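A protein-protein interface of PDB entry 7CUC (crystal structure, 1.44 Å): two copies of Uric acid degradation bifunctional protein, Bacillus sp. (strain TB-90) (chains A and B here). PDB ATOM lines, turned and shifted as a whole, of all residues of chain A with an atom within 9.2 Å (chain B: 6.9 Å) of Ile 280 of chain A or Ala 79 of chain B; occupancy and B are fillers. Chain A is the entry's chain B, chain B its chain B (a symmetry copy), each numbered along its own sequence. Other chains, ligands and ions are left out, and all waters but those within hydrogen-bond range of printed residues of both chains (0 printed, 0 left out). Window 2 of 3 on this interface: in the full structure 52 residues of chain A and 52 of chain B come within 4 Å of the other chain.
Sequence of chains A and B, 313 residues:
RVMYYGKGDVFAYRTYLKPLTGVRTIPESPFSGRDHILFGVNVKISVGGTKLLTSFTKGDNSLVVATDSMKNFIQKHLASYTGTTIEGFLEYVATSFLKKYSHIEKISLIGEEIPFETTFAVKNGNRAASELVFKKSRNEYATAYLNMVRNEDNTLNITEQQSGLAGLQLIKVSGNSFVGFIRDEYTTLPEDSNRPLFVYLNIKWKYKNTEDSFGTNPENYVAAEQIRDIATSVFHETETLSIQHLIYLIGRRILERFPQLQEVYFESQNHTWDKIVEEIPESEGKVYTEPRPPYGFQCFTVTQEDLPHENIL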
ATOM      1  N   ILE A 276     -12.389 -33.223 -20.104  1.00  0.00           N
ATOM      2  CA  ILE A 276     -12.303 -33.746 -18.747  1.00  0.00           C
ATOM      3  C   ILE A 276     -13.536 -33.371 -17.935  1.00  0.00           C
ATOM      4  O   ILE A 276     -14.190 -34.238 -17.335  1.00  0.00           O
ATOM      5  CB  ILE A 276     -11.029 -33.240 -18.034  1.00  0.00           C
ATOM      6  CG1 ILE A 276      -9.760 -33.792 -18.684  1.00  0.00           C
ATOM      7  CG2 ILE A 276     -11.068 -33.632 -16.571  1.00  0.00           C
ATOM      8  CD1 ILE A 276      -9.809 -35.283 -18.971  1.00  0.00           C
ATOM      9  N   VAL A 277     -13.883 -32.083 -17.914  1.00  0.00           N
ATOM     10  CA  VAL A 277     -15.046 -31.580 -17.188  1.00  0.00           C
ATOM     11  C   VAL A 277     -15.971 -30.887 -18.174  1.00  0.00           C
ATOM     12  O   VAL A 277     -15.580 -29.896 -18.805  1.00  0.00           O
ATOM     13  CB  VAL A 277     -14.651 -30.610 -16.060  1.00  0.00           C
ATOM     14  CG1 VAL A 277     -15.901 -30.118 -15.306  1.00  0.00           C
ATOM     15  CG2 VAL A 277     -13.665 -31.264 -15.094  1.00  0.00           C
ATOM     16  N   GLU A 278     -17.211 -31.384 -18.274  1.00  0.00           N
ATOM     17  CA  GLU A 278     -18.209 -30.837 -19.187  1.00  0.00           C
ATOM     18  C   GLU A 278     -19.022 -29.711 -18.561  1.00  0.00           C
ATOM     19  O   GLU A 278     -19.317 -28.717 -19.233  1.00  0.00           O
ATOM     20  CB  GLU A 278     -19.171 -31.942 -19.646  1.00  0.00           C
ATOM     21  N   GLU A 279     -19.392 -29.845 -17.289  1.00  0.00           N
ATOM     22  CA  GLU A 279     -20.269 -28.893 -16.618  1.00  0.00           C
ATOM     23  C   GLU A 279     -19.539 -28.275 -15.434  1.00  0.00           C
ATOM     24  O   GLU A 279     -19.078 -28.995 -14.542  1.00  0.00           O
ATOM     25  CB  GLU A 279     -21.546 -29.584 -16.132  1.00  0.00           C
ATOM     26  N   ILE A 280     -19.457 -26.948 -15.417  1.00  0.00           N
ATOM     27  CA  ILE A 280     -18.874 -26.195 -14.313  1.00  0.00           C
ATOM     28  C   ILE A 280     -19.985 -25.352 -13.700  1.00  0.00           C
ATOM     29  O   ILE A 280     -20.719 -24.688 -14.435  1.00  0.00           O
ATOM     30  CB  ILE A 280     -17.704 -25.302 -14.762  1.00  0.00           C
ATOM     31  CG1 ILE A 280     -16.567 -26.188 -15.283  1.00  0.00           C
ATOM     32  CG2 ILE A 280     -17.251 -24.426 -13.608  1.00  0.00           C
ATOM     33  CD1 ILE A 280     -15.350 -25.435 -15.787  1.00  0.00           C
ATOM     34  N   PRO A 281     -20.147 -25.344 -12.376  1.00  0.00           N
ATOM     35  CA  PRO A 281     -21.303 -24.656 -11.783  1.00  0.00           C
ATOM     36  C   PRO A 281     -21.251 -23.150 -12.012  1.00  0.00           C
ATOM     37  O   PRO A 281     -20.216 -22.510 -11.814  1.00  0.00           O
ATOM     38  CB  PRO A 281     -21.204 -25.010 -10.294  1.00  0.00           C
ATOM     39  N   GLU A 282     -22.385 -22.595 -12.436  1.00  0.00           N
ATOM     40  CA  GLU A 282     -22.550 -21.154 -12.611  1.00  0.00           C
ATOM     41  C   GLU A 282     -21.460 -20.541 -13.482  1.00  0.00           C
ATOM     42  O   GLU A 282     -20.970 -19.447 -13.198  1.00  0.00           O
ATOM     43  CB  GLU A 282     -22.584 -20.459 -11.244  1.00  0.00           C
ATOM     44  N   GLU A 284     -19.888 -20.923 -17.945  1.00  0.00           N
ATOM     45  CA  GLU A 284     -19.897 -21.515 -19.276  1.00  0.00           C
ATOM     46  C   GLU A 284     -18.600 -22.256 -19.620  1.00  0.00           C
ATOM     47  O   GLU A 284     -18.452 -22.757 -20.736  1.00  0.00           O
ATOM     48  CB  GLU A 284     -20.158 -20.426 -20.329  1.00  0.00           C
ATOM     49  N   GLY A 285     -17.671 -22.340 -18.650  1.00  0.00           N
ATOM     50  CA  GLY A 285     -16.374 -22.944 -18.906  1.00  0.00           C
ATOM     51  C   GLY A 285     -16.372 -24.468 -18.808  1.00  0.00           C
ATOM     52  O   GLY A 285     -17.302 -25.110 -18.328  1.00  0.00           O
ATOM     53  N   LYS A 286     -15.268 -25.049 -19.269  1.00  0.00           N
ATOM     54  CA  LYS A 286     -15.045 -26.487 -19.249  1.00  0.00           C
ATOM     55  C   LYS A 286     -13.561 -26.689 -18.952  1.00  0.00           C
ATOM     56  O   LYS A 286     -12.789 -25.723 -18.951  1.00  0.00           O
ATOM     57  CB  LYS A 286     -15.400 -27.074 -20.619  1.00  0.00           C
ATOM     58  CG  LYS A 286     -16.881 -26.875 -21.039  1.00  0.00           C
ATOM     59  N   VAL A 287     -13.133 -27.939 -18.752  1.00  0.00           N
ATOM     60  CA  VAL A 287     -11.697 -28.255 -18.656  1.00  0.00           C
ATOM     61  C   VAL A 287     -11.311 -29.366 -19.623  1.00  0.00           C
ATOM     62  O   VAL A 287     -11.999 -30.390 -19.739  1.00  0.00           O
ATOM     63  CB  VAL A 287     -11.275 -28.622 -17.218  1.00  0.00           C
ATOM     64  CG1 VAL A 287      -9.787 -29.003 -17.153  1.00  0.00           C
ATOM     65  CG2 VAL A 287     -11.547 -27.478 -16.272  1.00  0.00           C
ATOM     66  N   TYR A 288     -10.163 -29.183 -20.271  1.00  0.00           N
ATOM     67  CA  TYR A 288      -9.640 -30.092 -21.268  1.00  0.00           C
ATOM     68  C   TYR A 288      -8.198 -30.430 -20.929  1.00  0.00           C
ATOM     69  O   TYR A 288      -7.583 -29.774 -20.097  1.00  0.00           O
ATOM     70  CB  TYR A 288      -9.664 -29.468 -22.650  1.00  0.00           C
ATOM     71  CG  TYR A 288     -10.998 -28.944 -23.068  1.00  0.00           C
ATOM     72  CD1 TYR A 288     -11.419 -27.666 -22.737  1.00  0.00           C
ATOM     73  CD2 TYR A 288     -11.838 -29.741 -23.826  1.00  0.00           C
ATOM     74  CE1 TYR A 288     -12.653 -27.197 -23.149  1.00  0.00           C
ATOM     75  CE2 TYR A 288     -13.069 -29.299 -24.231  1.00  0.00           C
ATOM     76  CZ  TYR A 288     -13.474 -28.033 -23.893  1.00  0.00           C
ATOM     77  OH  TYR A 288     -14.694 -27.548 -24.291  1.00  0.00           O
ATOM     78  N   ARG B  14      -8.678 -24.441 -19.277  1.00  0.00           N
ATOM     79  CA  ARG B  14      -9.931 -23.985 -18.702  1.00  0.00           C
ATOM     80  C   ARG B  14     -10.439 -22.858 -19.588  1.00  0.00           C
ATOM     81  O   ARG B  14      -9.674 -21.980 -19.974  1.00  0.00           O
ATOM     82  CB  ARG B  14      -9.728 -23.497 -17.251  1.00  0.00           C
ATOM     83  CG  ARG B  14     -10.813 -22.627 -16.673  1.00  0.00           C
ATOM     84  CD  ARG B  14     -12.003 -23.398 -16.153  1.00  0.00           C
ATOM     85  NE  ARG B  14     -13.045 -22.446 -15.788  1.00  0.00           N
ATOM     86  CZ  ARG B  14     -13.319 -22.040 -14.552  1.00  0.00           C
ATOM     87  NH1 ARG B  14     -12.670 -22.528 -13.511  1.00  0.00           N
ATOM     88  NH2 ARG B  14     -14.279 -21.135 -14.361  1.00  0.00           N
ATOM     89  N   THR B  15     -11.716 -22.889 -19.938  1.00  0.00           N
ATOM     90  CA  THR B  15     -12.324 -21.756 -20.602  1.00  0.00           C
ATOM     91  C   THR B  15     -13.100 -20.904 -19.601  1.00  0.00           C
ATOM     92  O   THR B  15     -13.624 -21.397 -18.588  1.00  0.00           O
ATOM     93  CB  THR B  15     -13.203 -22.190 -21.773  1.00  0.00           C
ATOM     94  OG1 THR B  15     -14.227 -23.077 -21.295  1.00  0.00           O
ATOM     95  CG2 THR B  15     -12.368 -22.876 -22.848  1.00  0.00           C
ATOM     96  N   TYR B  16     -13.102 -19.599 -19.863  1.00  0.00           N
ATOM     97  CA  TYR B  16     -13.875 -18.625 -19.073  1.00  0.00           C
ATOM     98  C   TYR B  16     -13.560 -18.675 -17.573  1.00  0.00           C
ATOM     99  O   TYR B  16     -14.448 -18.743 -16.730  1.00  0.00           O
ATOM    100  CB  TYR B  16     -15.388 -18.711 -19.372  1.00  0.00           C
ATOM    101  CG  TYR B  16     -15.642 -18.631 -20.864  1.00  0.00           C
ATOM    102  CD1 TYR B  16     -15.531 -17.417 -21.529  1.00  0.00           C
ATOM    103  CD2 TYR B  16     -15.907 -19.767 -21.619  1.00  0.00           C
ATOM    104  CE1 TYR B  16     -15.709 -17.321 -22.906  1.00  0.00           C
ATOM    105  CE2 TYR B  16     -16.086 -19.684 -23.002  1.00  0.00           C
ATOM    106  CZ  TYR B  16     -15.982 -18.458 -23.637  1.00  0.00           C
ATOM    107  OH  TYR B  16     -16.138 -18.374 -25.006  1.00  0.00           O
ATOM    108  N   LEU B  17     -12.264 -18.576 -17.238  1.00  0.00           N
ATOM    109  CA  LEU B  17     -11.859 -18.258 -15.869  1.00  0.00           C
ATOM    110  C   LEU B  17     -12.270 -16.823 -15.556  1.00  0.00           C
ATOM    111  O   LEU B  17     -12.489 -16.009 -16.457  1.00  0.00           O
ATOM    112  CB  LEU B  17     -10.351 -18.467 -15.695  1.00  0.00           C
ATOM    113  CG  LEU B  17      -9.811 -18.481 -14.257  1.00  0.00           C
ATOM    114  CD1 LEU B  17     -10.189 -19.833 -13.654  1.00  0.00           C
ATOM    115  CD2 LEU B  17      -8.311 -18.260 -14.187  1.00  0.00           C
ATOM    116  N   ILE B  74      -6.006 -32.309  -9.746  1.00  0.00           N
ATOM    117  CA  ILE B  74      -5.640 -31.008 -10.312  1.00  0.00           C
ATOM    118  C   ILE B  74      -6.651 -30.563 -11.360  1.00  0.00           C
ATOM    119  O   ILE B  74      -7.095 -29.411 -11.369  1.00  0.00           O
ATOM    120  CB  ILE B  74      -4.221 -31.069 -10.905  1.00  0.00           C
ATOM    121  CG1 ILE B  74      -3.161 -31.244  -9.800  1.00  0.00           C
ATOM    122  CG2 ILE B  74      -3.916 -29.826 -11.768  1.00  0.00           C
ATOM    123  CD1 ILE B  74      -1.857 -31.756 -10.303  1.00  0.00           C
ATOM    124  N   GLN B  75      -6.989 -31.460 -12.285  1.00  0.00           N
ATOM    125  CA  GLN B  75      -7.919 -31.143 -13.362  1.00  0.00           C
ATOM    126  C   GLN B  75      -9.290 -30.786 -12.816  1.00  0.00           C
ATOM    127  O   GLN B  75      -9.894 -29.797 -13.237  1.00  0.00           O
ATOM    128  CB  GLN B  75      -7.949 -32.316 -14.353  1.00  0.00           C
ATOM    129  CG  GLN B  75      -6.554 -32.443 -15.021  1.00  0.00           C
ATOM    130  CD  GLN B  75      -6.436 -33.584 -16.008  1.00  0.00           C
ATOM    131  OE1 GLN B  75      -7.158 -34.573 -15.927  1.00  0.00           O
ATOM    132  NE2 GLN B  75      -5.480 -33.467 -16.933  1.00  0.00           N
ATOM    133  N   LYS B  76      -9.768 -31.531 -11.824  1.00  0.00           N
ATOM    134  CA  LYS B  76     -11.071 -31.206 -11.268  1.00  0.00           C
ATOM    135  C   LYS B  76     -11.042 -29.860 -10.544  1.00  0.00           C
ATOM    136  O   LYS B  76     -11.992 -29.077 -10.629  1.00  0.00           O
ATOM    137  CB  LYS B  76     -11.515 -32.324 -10.317  1.00  0.00           C
ATOM    138  CG  LYS B  76     -12.054 -33.537 -11.031  1.00  0.00           C
ATOM    139  CD  LYS B  76     -12.349 -34.657 -10.039  1.00  0.00           C
ATOM    140  CE  LYS B  76     -13.424 -35.622 -10.525  1.00  0.00           C
ATOM    141  NZ  LYS B  76     -13.878 -36.491  -9.392  1.00  0.00           N
ATOM    142  N   HIS B  77      -9.950 -29.562  -9.833  1.00  0.00           N
ATOM    143  CA  HIS B  77      -9.886 -28.284  -9.134  1.00  0.00           C
ATOM    144  C   HIS B  77      -9.730 -27.097 -10.078  1.00  0.00           C
ATOM    145  O   HIS B  77     -10.133 -25.973  -9.725  1.00  0.00           O
ATOM    146  CB  HIS B  77      -8.775 -28.335  -8.093  1.00  0.00           C
ATOM    147  CG  HIS B  77      -9.192 -29.004  -6.838  1.00  0.00           C
ATOM    148  ND1 HIS B  77      -9.394 -30.368  -6.773  1.00  0.00           N
ATOM    149  CD2 HIS B  77      -9.525 -28.513  -5.626  1.00  0.00           C
ATOM    150  CE1 HIS B  77      -9.794 -30.689  -5.554  1.00  0.00           C
ATOM    151  NE2 HIS B  77      -9.885 -29.581  -4.840  1.00  0.00           N
ATOM    152  N   LEU B  78      -9.203 -27.294 -11.287  1.00  0.00           N
ATOM    153  CA  LEU B  78      -9.206 -26.173 -12.219  1.00  0.00           C
ATOM    154  C   LEU B  78     -10.625 -25.836 -12.627  1.00  0.00           C
ATOM    155  O   LEU B  78     -10.935 -24.670 -12.904  1.00  0.00           O
ATOM    156  CB  LEU B  78      -8.361 -26.458 -13.467  1.00  0.00           C
ATOM    157  CG  LEU B  78      -8.218 -25.247 -14.402  1.00  0.00           C
ATOM    158  CD1 LEU B  78      -7.611 -24.055 -13.708  1.00  0.00           C
ATOM    159  CD2 LEU B  78      -7.352 -25.589 -15.580  1.00  0.00           C
ATOM    160  N   ALA B  79     -11.487 -26.852 -12.707  1.00  0.00           N
ATOM    161  CA  ALA B  79     -12.890 -26.608 -13.033  1.00  0.00           C
ATOM    162  C   ALA B  79     -13.593 -25.806 -11.934  1.00  0.00           C
ATOM    163  O   ALA B  79     -14.486 -25.004 -12.225  1.00  0.00           O
ATOM    164  CB  ALA B  79     -13.640 -27.939 -13.244  1.00  0.00           C
ATOM    165  N   SER B  80     -13.256 -26.039 -10.667  1.00  0.00           N
ATOM    166  CA  SER B  80     -13.945 -25.354  -9.574  1.00  0.00           C
ATOM    167  C   SER B  80     -13.263 -24.061  -9.108  1.00  0.00           C
ATOM    168  O   SER B  80     -13.848 -23.312  -8.322  1.00  0.00           O
ATOM    169  CB  SER B  80     -14.156 -26.294  -8.381  1.00  0.00           C
ATOM    170  OG  SER B  80     -12.935 -26.859  -7.957  1.00  0.00           O
ATOM    171  N   TYR B  81     -12.057 -23.772  -9.596  1.00  0.00           N
ATOM    172  CA  TYR B  81     -11.306 -22.619  -9.126  1.00  0.00           C
ATOM    173  C   TYR B  81     -12.024 -21.324  -9.508  1.00  0.00           C
ATOM    174  O   TYR B  81     -12.398 -21.118 -10.661  1.00  0.00           O
ATOM    175  CB  TYR B  81      -9.904 -22.648  -9.748  1.00  0.00           C
ATOM    176  CG  TYR B  81      -9.038 -21.489  -9.375  1.00  0.00           C
ATOM    177  CD1 TYR B  81      -8.877 -21.116  -8.057  1.00  0.00           C
ATOM    178  CD2 TYR B  81      -8.411 -20.752 -10.346  1.00  0.00           C
ATOM    179  CE1 TYR B  81      -8.078 -20.042  -7.710  1.00  0.00           C
ATOM    180  CE2 TYR B  81      -7.614 -19.657 -10.011  1.00  0.00           C
ATOM    181  CZ  TYR B  81      -7.455 -19.325  -8.701  1.00  0.00           C
ATOM    182  OH  TYR B  81      -6.673 -18.239  -8.381  1.00  0.00           O
ATOM    183  N   THR B  82     -12.179 -20.422  -8.534  1.00  0.00           N
ATOM    184  CA  THR B  82     -12.915 -19.177  -8.755  1.00  0.00           C
ATOM    185  C   THR B  82     -12.030 -17.945  -8.785  1.00  0.00           C
ATOM    186  O   THR B  82     -12.556 -16.826  -8.832  1.00  0.00           O
ATOM    187  CB  THR B  82     -13.998 -19.008  -7.696  1.00  0.00           C
ATOM    188  OG1 THR B  82     -13.396 -18.902  -6.404  1.00  0.00           O
ATOM    189  CG2 THR B  82     -14.916 -20.186  -7.706  1.00  0.00           C
ATOM    190  N   PHE B  89      -4.347 -20.408  -8.061  1.00  0.00           N
ATOM    191  CA  PHE B  89      -4.731 -21.773  -8.374  1.00  0.00           C
ATOM    192  C   PHE B  89      -3.869 -22.748  -7.592  1.00  0.00           C
ATOM    193  O   PHE B  89      -4.374 -23.723  -7.030  1.00  0.00           O
ATOM    194  CB  PHE B  89      -4.637 -22.043  -9.890  1.00  0.00           C
ATOM    195  CG  PHE B  89      -4.976 -23.458 -10.255  1.00  0.00           C
ATOM    196  CD1 PHE B  89      -6.226 -24.003  -9.921  1.00  0.00           C
ATOM    197  CD2 PHE B  89      -4.071 -24.255 -10.919  1.00  0.00           C
ATOM    198  CE1 PHE B  89      -6.528 -25.334 -10.228  1.00  0.00           C
ATOM    199  CE2 PHE B  89      -4.395 -25.567 -11.236  1.00  0.00           C
ATOM    200  CZ  PHE B  89      -5.606 -26.102 -10.868  1.00  0.00           C
ATOM    201  N   TYR B  92      -5.049 -22.935  -4.070  1.00  0.00           N
ATOM    202  CA  TYR B  92      -6.311 -23.661  -3.984  1.00  0.00           C
ATOM    203  C   TYR B  92      -6.080 -25.168  -4.033  1.00  0.00           C
ATOM    204  O   TYR B  92      -6.629 -25.929  -3.217  1.00  0.00           O
ATOM    205  CB  TYR B  92      -7.210 -23.175  -5.130  1.00  0.00           C
ATOM    206  CG  TYR B  92      -8.555 -23.869  -5.260  1.00  0.00           C
ATOM    207  CD1 TYR B  92      -9.462 -23.919  -4.195  1.00  0.00           C
ATOM    208  CD2 TYR B  92      -8.953 -24.435  -6.470  1.00  0.00           C
ATOM    209  CE1 TYR B  92     -10.700 -24.543  -4.318  1.00  0.00           C
ATOM    210  CE2 TYR B  92     -10.188 -25.061  -6.591  1.00  0.00           C
ATOM    211  CZ  TYR B  92     -11.053 -25.112  -5.513  1.00  0.00           C
ATOM    212  OH  TYR B  92     -12.288 -25.718  -5.621  1.00  0.00           O
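No position is printed for both chains. Of the 9 pairs that touch across the chains among the printed residues, none has its exchanged pair printed and touching as well.
Ile 280 of chain A touches two residues of chain B. Of the printed residues of chain A, Ala 79 of chain B touches Val 277 (3.8 Å), Ile 280 (3.1 Å) and Val 287 (3.6 Å). Ser 80 of chain B touches none of the printed residues of chain A. Printed residues of chain A within 4 Å of Arg 14 of chain B: Ile 280 (3.8 Å) and Lys 286 (3.4 Å). Of the printed residues of chain A, Thr 15 of chain B touches Gly 285 (3.2 Å) and Lys 286 (3.0 Å). Of the printed residues of chain A, Gln 75 of chain B touches Ile 276 (3.9 Å) and Val 287 (3.997 Å). Printed residues of chain B within 4 Å of Ile 276 of chain A: Gln 75 (3.9 Å). Leu 78 of chain B touches none of the printed residues of chain A. The nearest printed residue of chain A that does not touch Arg 14 of chain B is Val 287 of chain A (4.1 Å).
N of Val 277 of chain A is in hydrogen-bond range of O of Val 287 of chain A, 3.1 Å away. O of Tyr 81 of chain B sits at hydrogen-bond distance from NH1 of Arg 14 of chain B. The guanidinium group of Arg 14 of chain B lies within hydrogen-bond range of the backbone carbonyl oxygen of Tyr 16 of chain B. The backbone NH of Ile 276 of chain A lies within hydrogen-bond range of the backbone carbonyl oxygen of Val 287 of chain A (2.9 Å). The guanidinium group (NH1) of Arg 14 of chain B lies within hydrogen-bond range of the backbone carbonyl oxygen (O) of Ala 79 of chain B (3.3 Å). The guanidinium group of Arg 14 of chain B lies within hydrogen-bond range of the backbone carbonyl oxygen of Leu 78 of chain B (2.8 Å).
Printed residues of chain A that touch a printed residue of chain B: Ile 276, Val 277, Ile 280, Gly 285, Lys 286 and Val 287. Among the printed residues, no Asp or Glu carboxylate lies within 4 Å of a Lys or Arg side-chain nitrogen of the other chain.
OG1 of Thr 15 of chain B sits at hydrogen-bond distance from N of Lys 286 of chain A (3.0 Å).
Ile 276 of chain A touches Gln 75 of chain B. Val 277 of chain A touches Ala 79 of chain B. Arg 14 of chain B touches Ile 280 of chain A. Ala 79 of chain B touches Ile 280 of chain A. Gly 285 of chain A touches Thr 15 of chain B (CA to O, 3.2 Å). CA of Arg 14 of chain B touches O of Lys 286 of chain A, at 3.4 Å. Gln 75 of chain B touches Val 287 of chain A (O to CG1, 3.997 Å). CA of Ala 79 of chain B touches CG2 of Val 287 of chain A, 3.6 Å away.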
